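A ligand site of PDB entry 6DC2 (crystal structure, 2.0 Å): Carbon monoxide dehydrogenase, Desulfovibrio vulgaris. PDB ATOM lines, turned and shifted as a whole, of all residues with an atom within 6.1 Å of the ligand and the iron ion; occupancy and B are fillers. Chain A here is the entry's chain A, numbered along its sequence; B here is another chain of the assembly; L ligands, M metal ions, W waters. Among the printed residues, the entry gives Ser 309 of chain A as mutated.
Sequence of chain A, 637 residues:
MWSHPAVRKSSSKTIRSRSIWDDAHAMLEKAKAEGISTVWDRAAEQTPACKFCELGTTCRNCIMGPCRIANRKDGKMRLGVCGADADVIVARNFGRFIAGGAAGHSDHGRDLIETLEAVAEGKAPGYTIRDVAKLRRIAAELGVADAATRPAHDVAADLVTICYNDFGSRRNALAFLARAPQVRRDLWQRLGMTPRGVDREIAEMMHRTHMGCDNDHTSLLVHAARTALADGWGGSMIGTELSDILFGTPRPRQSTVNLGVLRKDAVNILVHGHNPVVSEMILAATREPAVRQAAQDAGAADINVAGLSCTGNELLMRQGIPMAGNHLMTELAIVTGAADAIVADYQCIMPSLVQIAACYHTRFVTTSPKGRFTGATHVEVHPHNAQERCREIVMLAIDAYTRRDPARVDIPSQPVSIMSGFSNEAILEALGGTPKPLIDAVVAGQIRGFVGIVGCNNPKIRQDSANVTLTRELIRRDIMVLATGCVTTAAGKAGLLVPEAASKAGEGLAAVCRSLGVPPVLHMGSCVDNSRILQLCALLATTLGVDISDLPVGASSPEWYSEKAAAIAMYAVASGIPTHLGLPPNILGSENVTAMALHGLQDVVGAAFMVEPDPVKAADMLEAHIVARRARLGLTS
Merely in contact with the iron ion: Cys 310.
Of the 24 residues printed, 2 come within 4 Å of the iron ion.
The nearest printed residue that does not touch the iron ion is His 274 (4.03 Å).
The backbone carbonyl oxygen (O) of Gly 455 sits close to a sulfur (S1) of the ligand (3.5 Å).
Residues that only touch the ligand: Ser 309, His 327 and Tyr 561.
Hydrophobic or aromatic side chains within 4 Å of the ligand: His 274, His 327 and Tyr 561.
The nearest printed residue that does not touch the ligand is Gly 485 (4.1 Å).
NE2 of His 274 binds FE2 of the ligand (2.2 Å).
SG of Cys 310 is bound to FE2 of the ligand, 2.4 Å away.
The side-chain sulfur of Cys 348 binds an iron atom (FE1) of the ligand.
FE3 of the ligand is bound by SG of Cys 456 (2.5 Å).
N of Cys 486 lies close to S1 of the ligand.
SG of Cys 486 is bound to FE4 of the ligand, 2.5 Å away.
OG of Ser 562 lies close to S3 of the ligand (3.1 Å).
NZ of Lys 564 lies close to S3 of the ligand, 3.4 Å away.
The iron ion is bound by S1 of the ligand (2.3 Å), SG of Cys 527 (2.4 Å), S3 of the ligand (2.6 Å) and S4 of the ligand (2.7 Å).
The iron ion has four donor atoms within binding distance.
Slightly farther from the iron ion lies water W1 (2.8 Å).
SG of Cys 310 lies close to N of Cys 527, at 3.4 Å.
The side-chain sulfur (SG) of Cys 348 lies close to the side-chain hydroxyl (OH) of Tyr 561 (3.2 Å).
The side-chain sulfur (SG) of Cys 348 lies close to the side-chain amino group (NZ) of Lys 564, at 3.4 Å.
The backbone NH (N) of Cys 486 is in hydrogen-bond range of the backbone carbonyl oxygen (O) of Gly 455 (3.3 Å).
The backbone carbonyl oxygen of Cys 486 is in hydrogen-bond range of the side-chain amide nitrogen of Asn 326, 3.0 Å away.
The backbone NH (N) of Ala 565 is in hydrogen-bond range of the side-chain hydroxyl (OG) of Ser 562, 3.2 Å away.
The side-chain amino group (NZ) of Lys 564 sits at hydrogen-bond distance from the side-chain amide oxygen (OE1) of Gln 347, 3.1 Å away.
N of Val 487 is in hydrogen-bond range of O of Gly 455 (3.3 Å).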
ATOM      1  N   GLY A 273      11.380 -12.467  17.586  1.00  0.00           N
ATOM      2  CA  GLY A 273      11.406 -13.635  16.740  1.00  0.00           C
ATOM      3  C   GLY A 273      11.379 -13.247  15.267  1.00  0.00           C
ATOM      4  O   GLY A 273      12.065 -12.303  14.856  1.00  0.00           O
ATOM      5  N   HIS A 274      10.563 -13.964  14.491  1.00  0.00           N
ATOM      6  CA  HIS A 274      10.701 -13.877  13.040  1.00  0.00           C
ATOM      7  C   HIS A 274       9.424 -13.830  12.199  1.00  0.00           C
ATOM      8  O   HIS A 274       9.410 -13.142  11.163  1.00  0.00           O
ATOM      9  CB  HIS A 274      11.640 -14.983  12.544  1.00  0.00           C
ATOM     10  CG  HIS A 274      13.074 -14.685  12.796  1.00  0.00           C
ATOM     11  ND1 HIS A 274      13.665 -14.834  14.029  1.00  0.00           N
ATOM     12  CD2 HIS A 274      14.042 -14.201  11.982  1.00  0.00           C
ATOM     13  CE1 HIS A 274      14.927 -14.470  13.965  1.00  0.00           C
ATOM     14  NE2 HIS A 274      15.183 -14.070  12.732  1.00  0.00           N
ATOM     15  N   SER A 309      14.194  -7.270  16.446  1.00  0.00           N
ATOM     16  CA  SER A 309      14.820  -8.193  15.481  1.00  0.00           C
ATOM     17  C   SER A 309      13.955  -8.297  14.216  1.00  0.00           C
ATOM     18  O   SER A 309      13.323  -7.312  13.804  1.00  0.00           O
ATOM     19  CB  SER A 309      15.173  -9.496  16.159  1.00  0.00           C
ATOM     20  OG  SER A 309      16.047  -9.245  17.249  1.00  0.00           O
ATOM     21  N   CYS A 310      13.902  -9.478  13.607  1.00  0.00           N
ATOM     22  CA  CYS A 310      13.347  -9.581  12.258  1.00  0.00           C
ATOM     23  C   CYS A 310      11.833  -9.442  12.240  1.00  0.00           C
ATOM     24  O   CYS A 310      11.266  -8.889  11.294  1.00  0.00           O
ATOM     25  CB  CYS A 310      13.778 -10.886  11.591  1.00  0.00           C
ATOM     26  SG  CYS A 310      15.390 -10.755  10.833  1.00  0.00           S
ATOM     27  N   ASN A 326      17.802  -4.254  18.054  1.00  0.00           N
ATOM     28  CA  ASN A 326      18.276  -5.443  17.374  1.00  0.00           C
ATOM     29  C   ASN A 326      18.832  -6.466  18.372  1.00  0.00           C
ATOM     30  O   ASN A 326      18.550  -6.378  19.581  1.00  0.00           O
ATOM     31  CB  ASN A 326      19.280  -5.036  16.282  1.00  0.00           C
ATOM     32  CG  ASN A 326      20.354  -4.101  16.804  1.00  0.00           C
ATOM     33  OD1 ASN A 326      20.411  -3.793  17.996  1.00  0.00           O
ATOM     34  ND2 ASN A 326      21.230  -3.655  15.905  1.00  0.00           N
ATOM     35  N   HIS A 327      19.631  -7.407  17.877  1.00  0.00           N
ATOM     36  CA  HIS A 327      19.965  -8.628  18.615  1.00  0.00           C
ATOM     37  C   HIS A 327      20.520  -8.343  20.012  1.00  0.00           C
ATOM     38  O   HIS A 327      20.012  -8.881  21.007  1.00  0.00           O
ATOM     39  CB  HIS A 327      20.936  -9.489  17.800  1.00  0.00           C
ATOM     40  CG  HIS A 327      21.429 -10.711  18.514  1.00  0.00           C
ATOM     41  ND1 HIS A 327      20.582 -11.604  19.133  1.00  0.00           N
ATOM     42  CD2 HIS A 327      22.676 -11.197  18.700  1.00  0.00           C
ATOM     43  CE1 HIS A 327      21.286 -12.587  19.674  1.00  0.00           C
ATOM     44  NE2 HIS A 327      22.565 -12.352  19.439  1.00  0.00           N
ATOM     45  N   GLN A 347      13.740 -18.487  16.640  1.00  0.00           N
ATOM     46  CA  GLN A 347      15.032 -18.069  16.097  1.00  0.00           C
ATOM     47  C   GLN A 347      15.587 -16.809  16.755  1.00  0.00           C
ATOM     48  O   GLN A 347      14.898 -15.784  16.812  1.00  0.00           O
ATOM     49  CB  GLN A 347      14.984 -17.911  14.570  1.00  0.00           C
ATOM     50  CG  GLN A 347      14.611 -19.179  13.827  1.00  0.00           C
ATOM     51  CD  GLN A 347      14.286 -18.890  12.375  1.00  0.00           C
ATOM     52  OE1 GLN A 347      14.566 -17.807  11.872  1.00  0.00           O
ATOM     53  NE2 GLN A 347      13.664 -19.861  11.705  1.00  0.00           N
ATOM     54  N   CYS A 348      16.824 -16.892  17.247  1.00  0.00           N
ATOM     55  CA  CYS A 348      17.601 -15.780  17.803  1.00  0.00           C
ATOM     56  C   CYS A 348      17.057 -15.256  19.119  1.00  0.00           C
ATOM     57  O   CYS A 348      17.496 -14.191  19.573  1.00  0.00           O
ATOM     58  CB  CYS A 348      17.782 -14.637  16.802  1.00  0.00           C
ATOM     59  SG  CYS A 348      18.436 -15.210  15.240  1.00  0.00           S
ATOM     60  N   VAL A 454      23.936  -6.748   5.805  1.00  0.00           N
ATOM     61  CA  VAL A 454      22.951  -7.674   6.352  1.00  0.00           C
ATOM     62  C   VAL A 454      23.495  -8.237   7.667  1.00  0.00           C
ATOM     63  O   VAL A 454      24.656  -8.065   8.011  1.00  0.00           O
ATOM     64  CB  VAL A 454      22.637  -8.805   5.361  1.00  0.00           C
ATOM     65  CG1 VAL A 454      22.280  -8.244   3.998  1.00  0.00           C
ATOM     66  CG2 VAL A 454      23.827  -9.747   5.238  1.00  0.00           C
ATOM     67  N   GLY A 455      22.623  -8.897   8.410  1.00  0.00           N
ATOM     68  CA  GLY A 455      23.083  -9.706   9.521  1.00  0.00           C
ATOM     69  C   GLY A 455      23.055  -9.005  10.867  1.00  0.00           C
ATOM     70  O   GLY A 455      22.425  -7.969  11.080  1.00  0.00           O
ATOM     71  N   CYS A 456      23.827  -9.589  11.785  1.00  0.00           N
ATOM     72  CA  CYS A 456      23.555  -9.611  13.211  1.00  0.00           C
ATOM     73  C   CYS A 456      24.383  -8.598  13.998  1.00  0.00           C
ATOM     74  O   CYS A 456      25.011  -7.691  13.441  1.00  0.00           O
ATOM     75  CB  CYS A 456      23.864 -11.014  13.739  1.00  0.00           C
ATOM     76  SG  CYS A 456      23.484 -12.367  12.591  1.00  0.00           S
ATOM     77  N   ASN A 457      24.350  -8.744  15.326  1.00  0.00           N
ATOM     78  CA  ASN A 457      25.382  -8.276  16.243  1.00  0.00           C
ATOM     79  C   ASN A 457      26.113  -9.498  16.788  1.00  0.00           C
ATOM     80  O   ASN A 457      25.631 -10.622  16.698  1.00  0.00           O
ATOM     81  CB  ASN A 457      24.768  -7.522  17.429  1.00  0.00           C
ATOM     82  CG  ASN A 457      23.991  -6.270  17.031  1.00  0.00           C
ATOM     83  OD1 ASN A 457      22.958  -5.963  17.622  1.00  0.00           O
ATOM     84  ND2 ASN A 457      24.495  -5.541  16.043  1.00  0.00           N
ATOM     85  N   THR A 484      19.097  -4.854   5.682  1.00  0.00           N
ATOM     86  CA  THR A 484      18.133  -5.838   6.173  1.00  0.00           C
ATOM     87  C   THR A 484      18.585  -6.349   7.528  1.00  0.00           C
ATOM     88  O   THR A 484      19.741  -6.184   7.936  1.00  0.00           O
ATOM     89  CB  THR A 484      18.014  -7.053   5.240  1.00  0.00           C
ATOM     90  OG1 THR A 484      19.241  -7.807   5.284  1.00  0.00           O
ATOM     91  CG2 THR A 484      17.712  -6.642   3.793  1.00  0.00           C
ATOM     92  N   GLY A 485      17.668  -7.003   8.226  1.00  0.00           N
ATOM     93  CA  GLY A 485      18.041  -7.679   9.458  1.00  0.00           C
ATOM     94  C   GLY A 485      18.370  -6.704  10.578  1.00  0.00           C
ATOM     95  O   GLY A 485      17.816  -5.601  10.665  1.00  0.00           O
ATOM     96  N   CYS A 486      19.282  -7.126  11.446  1.00  0.00           N
ATOM     97  CA  CYS A 486      19.638  -6.286  12.590  1.00  0.00           C
ATOM     98  C   CYS A 486      20.482  -5.077  12.203  1.00  0.00           C
ATOM     99  O   CYS A 486      20.670  -4.179  13.027  1.00  0.00           O
ATOM    100  CB  CYS A 486      20.325  -7.122  13.665  1.00  0.00           C
ATOM    101  SG  CYS A 486      19.168  -8.127  14.621  1.00  0.00           S
ATOM    102  N   VAL A 487      20.975  -5.023  10.969  1.00  0.00           N
ATOM    103  CA  VAL A 487      21.646  -3.817  10.492  1.00  0.00           C
ATOM    104  C   VAL A 487      20.659  -2.650  10.382  1.00  0.00           C
ATOM    105  O   VAL A 487      21.048  -1.487  10.562  1.00  0.00           O
ATOM    106  CB  VAL A 487      22.371  -4.126   9.167  1.00  0.00           C
ATOM    107  CG1 VAL A 487      23.004  -2.872   8.594  1.00  0.00           C
ATOM    108  CG2 VAL A 487      23.421  -5.210   9.400  1.00  0.00           C
ATOM    109  N   SER A 526      13.462  -7.950   6.526  1.00  0.00           N
ATOM    110  CA  SER A 526      14.023  -8.888   7.488  1.00  0.00           C
ATOM    111  C   SER A 526      15.103  -9.727   6.816  1.00  0.00           C
ATOM    112  O   SER A 526      15.560  -9.434   5.702  1.00  0.00           O
ATOM    113  CB  SER A 526      12.910  -9.783   8.018  1.00  0.00           C
ATOM    114  OG  SER A 526      12.289 -10.458   6.940  1.00  0.00           O
ATOM    115  N   CYS A 527      15.533 -10.808   7.484  1.00  0.00           N
ATOM    116  CA  CYS A 527      16.565 -11.652   6.903  1.00  0.00           C
ATOM    117  C   CYS A 527      16.040 -12.489   5.749  1.00  0.00           C
ATOM    118  O   CYS A 527      16.754 -12.720   4.765  1.00  0.00           O
ATOM    119  CB  CYS A 527      17.209 -12.537   7.967  1.00  0.00           C
ATOM    120  SG  CYS A 527      18.294 -11.617   9.056  1.00  0.00           S
ATOM    121  N   TYR A 561      26.563 -13.491  13.573  1.00  0.00           N
ATOM    122  CA  TYR A 561      26.738 -14.549  14.561  1.00  0.00           C
ATOM    123  C   TYR A 561      26.099 -15.880  14.167  1.00  0.00           C
ATOM    124  O   TYR A 561      26.623 -16.920  14.571  1.00  0.00           O
ATOM    125  CB  TYR A 561      26.200 -14.128  15.966  1.00  0.00           C
ATOM    126  CG  TYR A 561      24.792 -14.661  16.232  1.00  0.00           C
ATOM    127  CD1 TYR A 561      24.589 -15.944  16.762  1.00  0.00           C
ATOM    128  CD2 TYR A 561      23.673 -13.887  15.949  1.00  0.00           C
ATOM    129  CE1 TYR A 561      23.320 -16.431  16.964  1.00  0.00           C
ATOM    130  CE2 TYR A 561      22.401 -14.382  16.171  1.00  0.00           C
ATOM    131  CZ  TYR A 561      22.230 -15.651  16.679  1.00  0.00           C
ATOM    132  OH  TYR A 561      20.967 -16.146  16.879  1.00  0.00           O
ATOM    133  N   SER A 562      24.999 -15.902  13.425  1.00  0.00           N
ATOM    134  CA  SER A 562      24.117 -17.056  13.355  1.00  0.00           C
ATOM    135  C   SER A 562      24.386 -17.954  12.151  1.00  0.00           C
ATOM    136  O   SER A 562      25.060 -17.584  11.187  1.00  0.00           O
ATOM    137  CB  SER A 562      22.660 -16.612  13.329  1.00  0.00           C
ATOM    138  OG  SER A 562      22.398 -15.876  12.140  1.00  0.00           O
ATOM    139  N   LYS A 564      21.994 -18.806  10.155  1.00  0.00           N
ATOM    140  CA  LYS A 564      21.239 -18.192   9.068  1.00  0.00           C
ATOM    141  C   LYS A 564      22.066 -17.159   8.318  1.00  0.00           C
ATOM    142  O   LYS A 564      21.997 -17.066   7.092  1.00  0.00           O
ATOM    143  CB  LYS A 564      19.950 -17.575   9.604  1.00  0.00           C
ATOM    144  CG  LYS A 564      18.926 -18.597  10.095  1.00  0.00           C
ATOM    145  CD  LYS A 564      17.710 -17.913  10.694  1.00  0.00           C
ATOM    146  CE  LYS A 564      18.076 -17.197  11.972  1.00  0.00           C
ATOM    147  NZ  LYS A 564      17.151 -16.067  12.218  1.00  0.00           N
ATOM    148  N   ALA A 565      22.862 -16.370   9.045  1.00  0.00           N
ATOM    149  CA  ALA A 565      23.692 -15.370   8.390  1.00  0.00           C
ATOM    150  C   ALA A 565      24.724 -16.023   7.483  1.00  0.00           C
ATOM    151  O   ALA A 565      25.016 -15.526   6.395  1.00  0.00           O
ATOM    152  CB  ALA A 565      24.375 -14.476   9.429  1.00  0.00           C
ATOM    153  N   ILE A 568      22.906 -17.109   4.352  1.00  0.00           N
ATOM    154  CA  ILE A 568      22.715 -15.937   3.495  1.00  0.00           C
ATOM    155  C   ILE A 568      24.004 -15.615   2.748  1.00  0.00           C
ATOM    156  O   ILE A 568      23.998 -15.398   1.531  1.00  0.00           O
ATOM    157  CB  ILE A 568      22.210 -14.728   4.312  1.00  0.00           C
ATOM    158  CG1 ILE A 568      20.793 -14.976   4.826  1.00  0.00           C
ATOM    159  CG2 ILE A 568      22.257 -13.444   3.473  1.00  0.00           C
ATOM    160  CD1 ILE A 568      20.465 -14.212   6.121  1.00  0.00           C
ATOM    161  N   HIS B 210      18.861 -24.593  15.889  1.00  0.00           N
ATOM    162  CA  HIS B 210      19.458 -23.277  15.699  1.00  0.00           C
ATOM    163  C   HIS B 210      19.329 -22.482  16.993  1.00  0.00           C
ATOM    164  O   HIS B 210      18.415 -22.722  17.796  1.00  0.00           O
ATOM    165  CB  HIS B 210      18.752 -22.567  14.545  1.00  0.00           C
ATOM    166  CG  HIS B 210      19.337 -21.242  14.148  1.00  0.00           C
ATOM    167  ND1 HIS B 210      19.258 -20.121  14.948  1.00  0.00           N
ATOM    168  CD2 HIS B 210      19.982 -20.850  13.018  1.00  0.00           C
ATOM    169  CE1 HIS B 210      19.838 -19.099  14.337  1.00  0.00           C
ATOM    170  NE2 HIS B 210      20.290 -19.521  13.158  1.00  0.00           N
HETATM  171 FE1  LIG L   1      19.058 -13.138  14.082  1.00  0.00          FE
HETATM  172 FE2  LIG L   1      16.620 -12.573  11.888  1.00  0.00          FE
HETATM  173 FE3  LIG L   1      21.028 -12.202  12.675  1.00  0.00          FE
HETATM  174 FE4  LIG L   1      19.297 -10.415  13.711  1.00  0.00          FE
HETATM  175  S1  LIG L   1      20.047 -10.459  11.637  1.00  0.00           S
HETATM  176  S2  LIG L   1      20.635 -11.788  14.960  1.00  0.00           S
HETATM  177  S3  LIG L   1      19.866 -14.024  12.129  1.00  0.00           S
HETATM  178  S4  LIG L   1      17.338 -11.660  13.860  1.00  0.00           S
HETATM  179 FE    FE M   1      18.402 -12.030  11.419  1.00  0.00          FE
HETATM  180  O   HOH W   1      16.707 -14.091  10.611  1.00  0.00           O
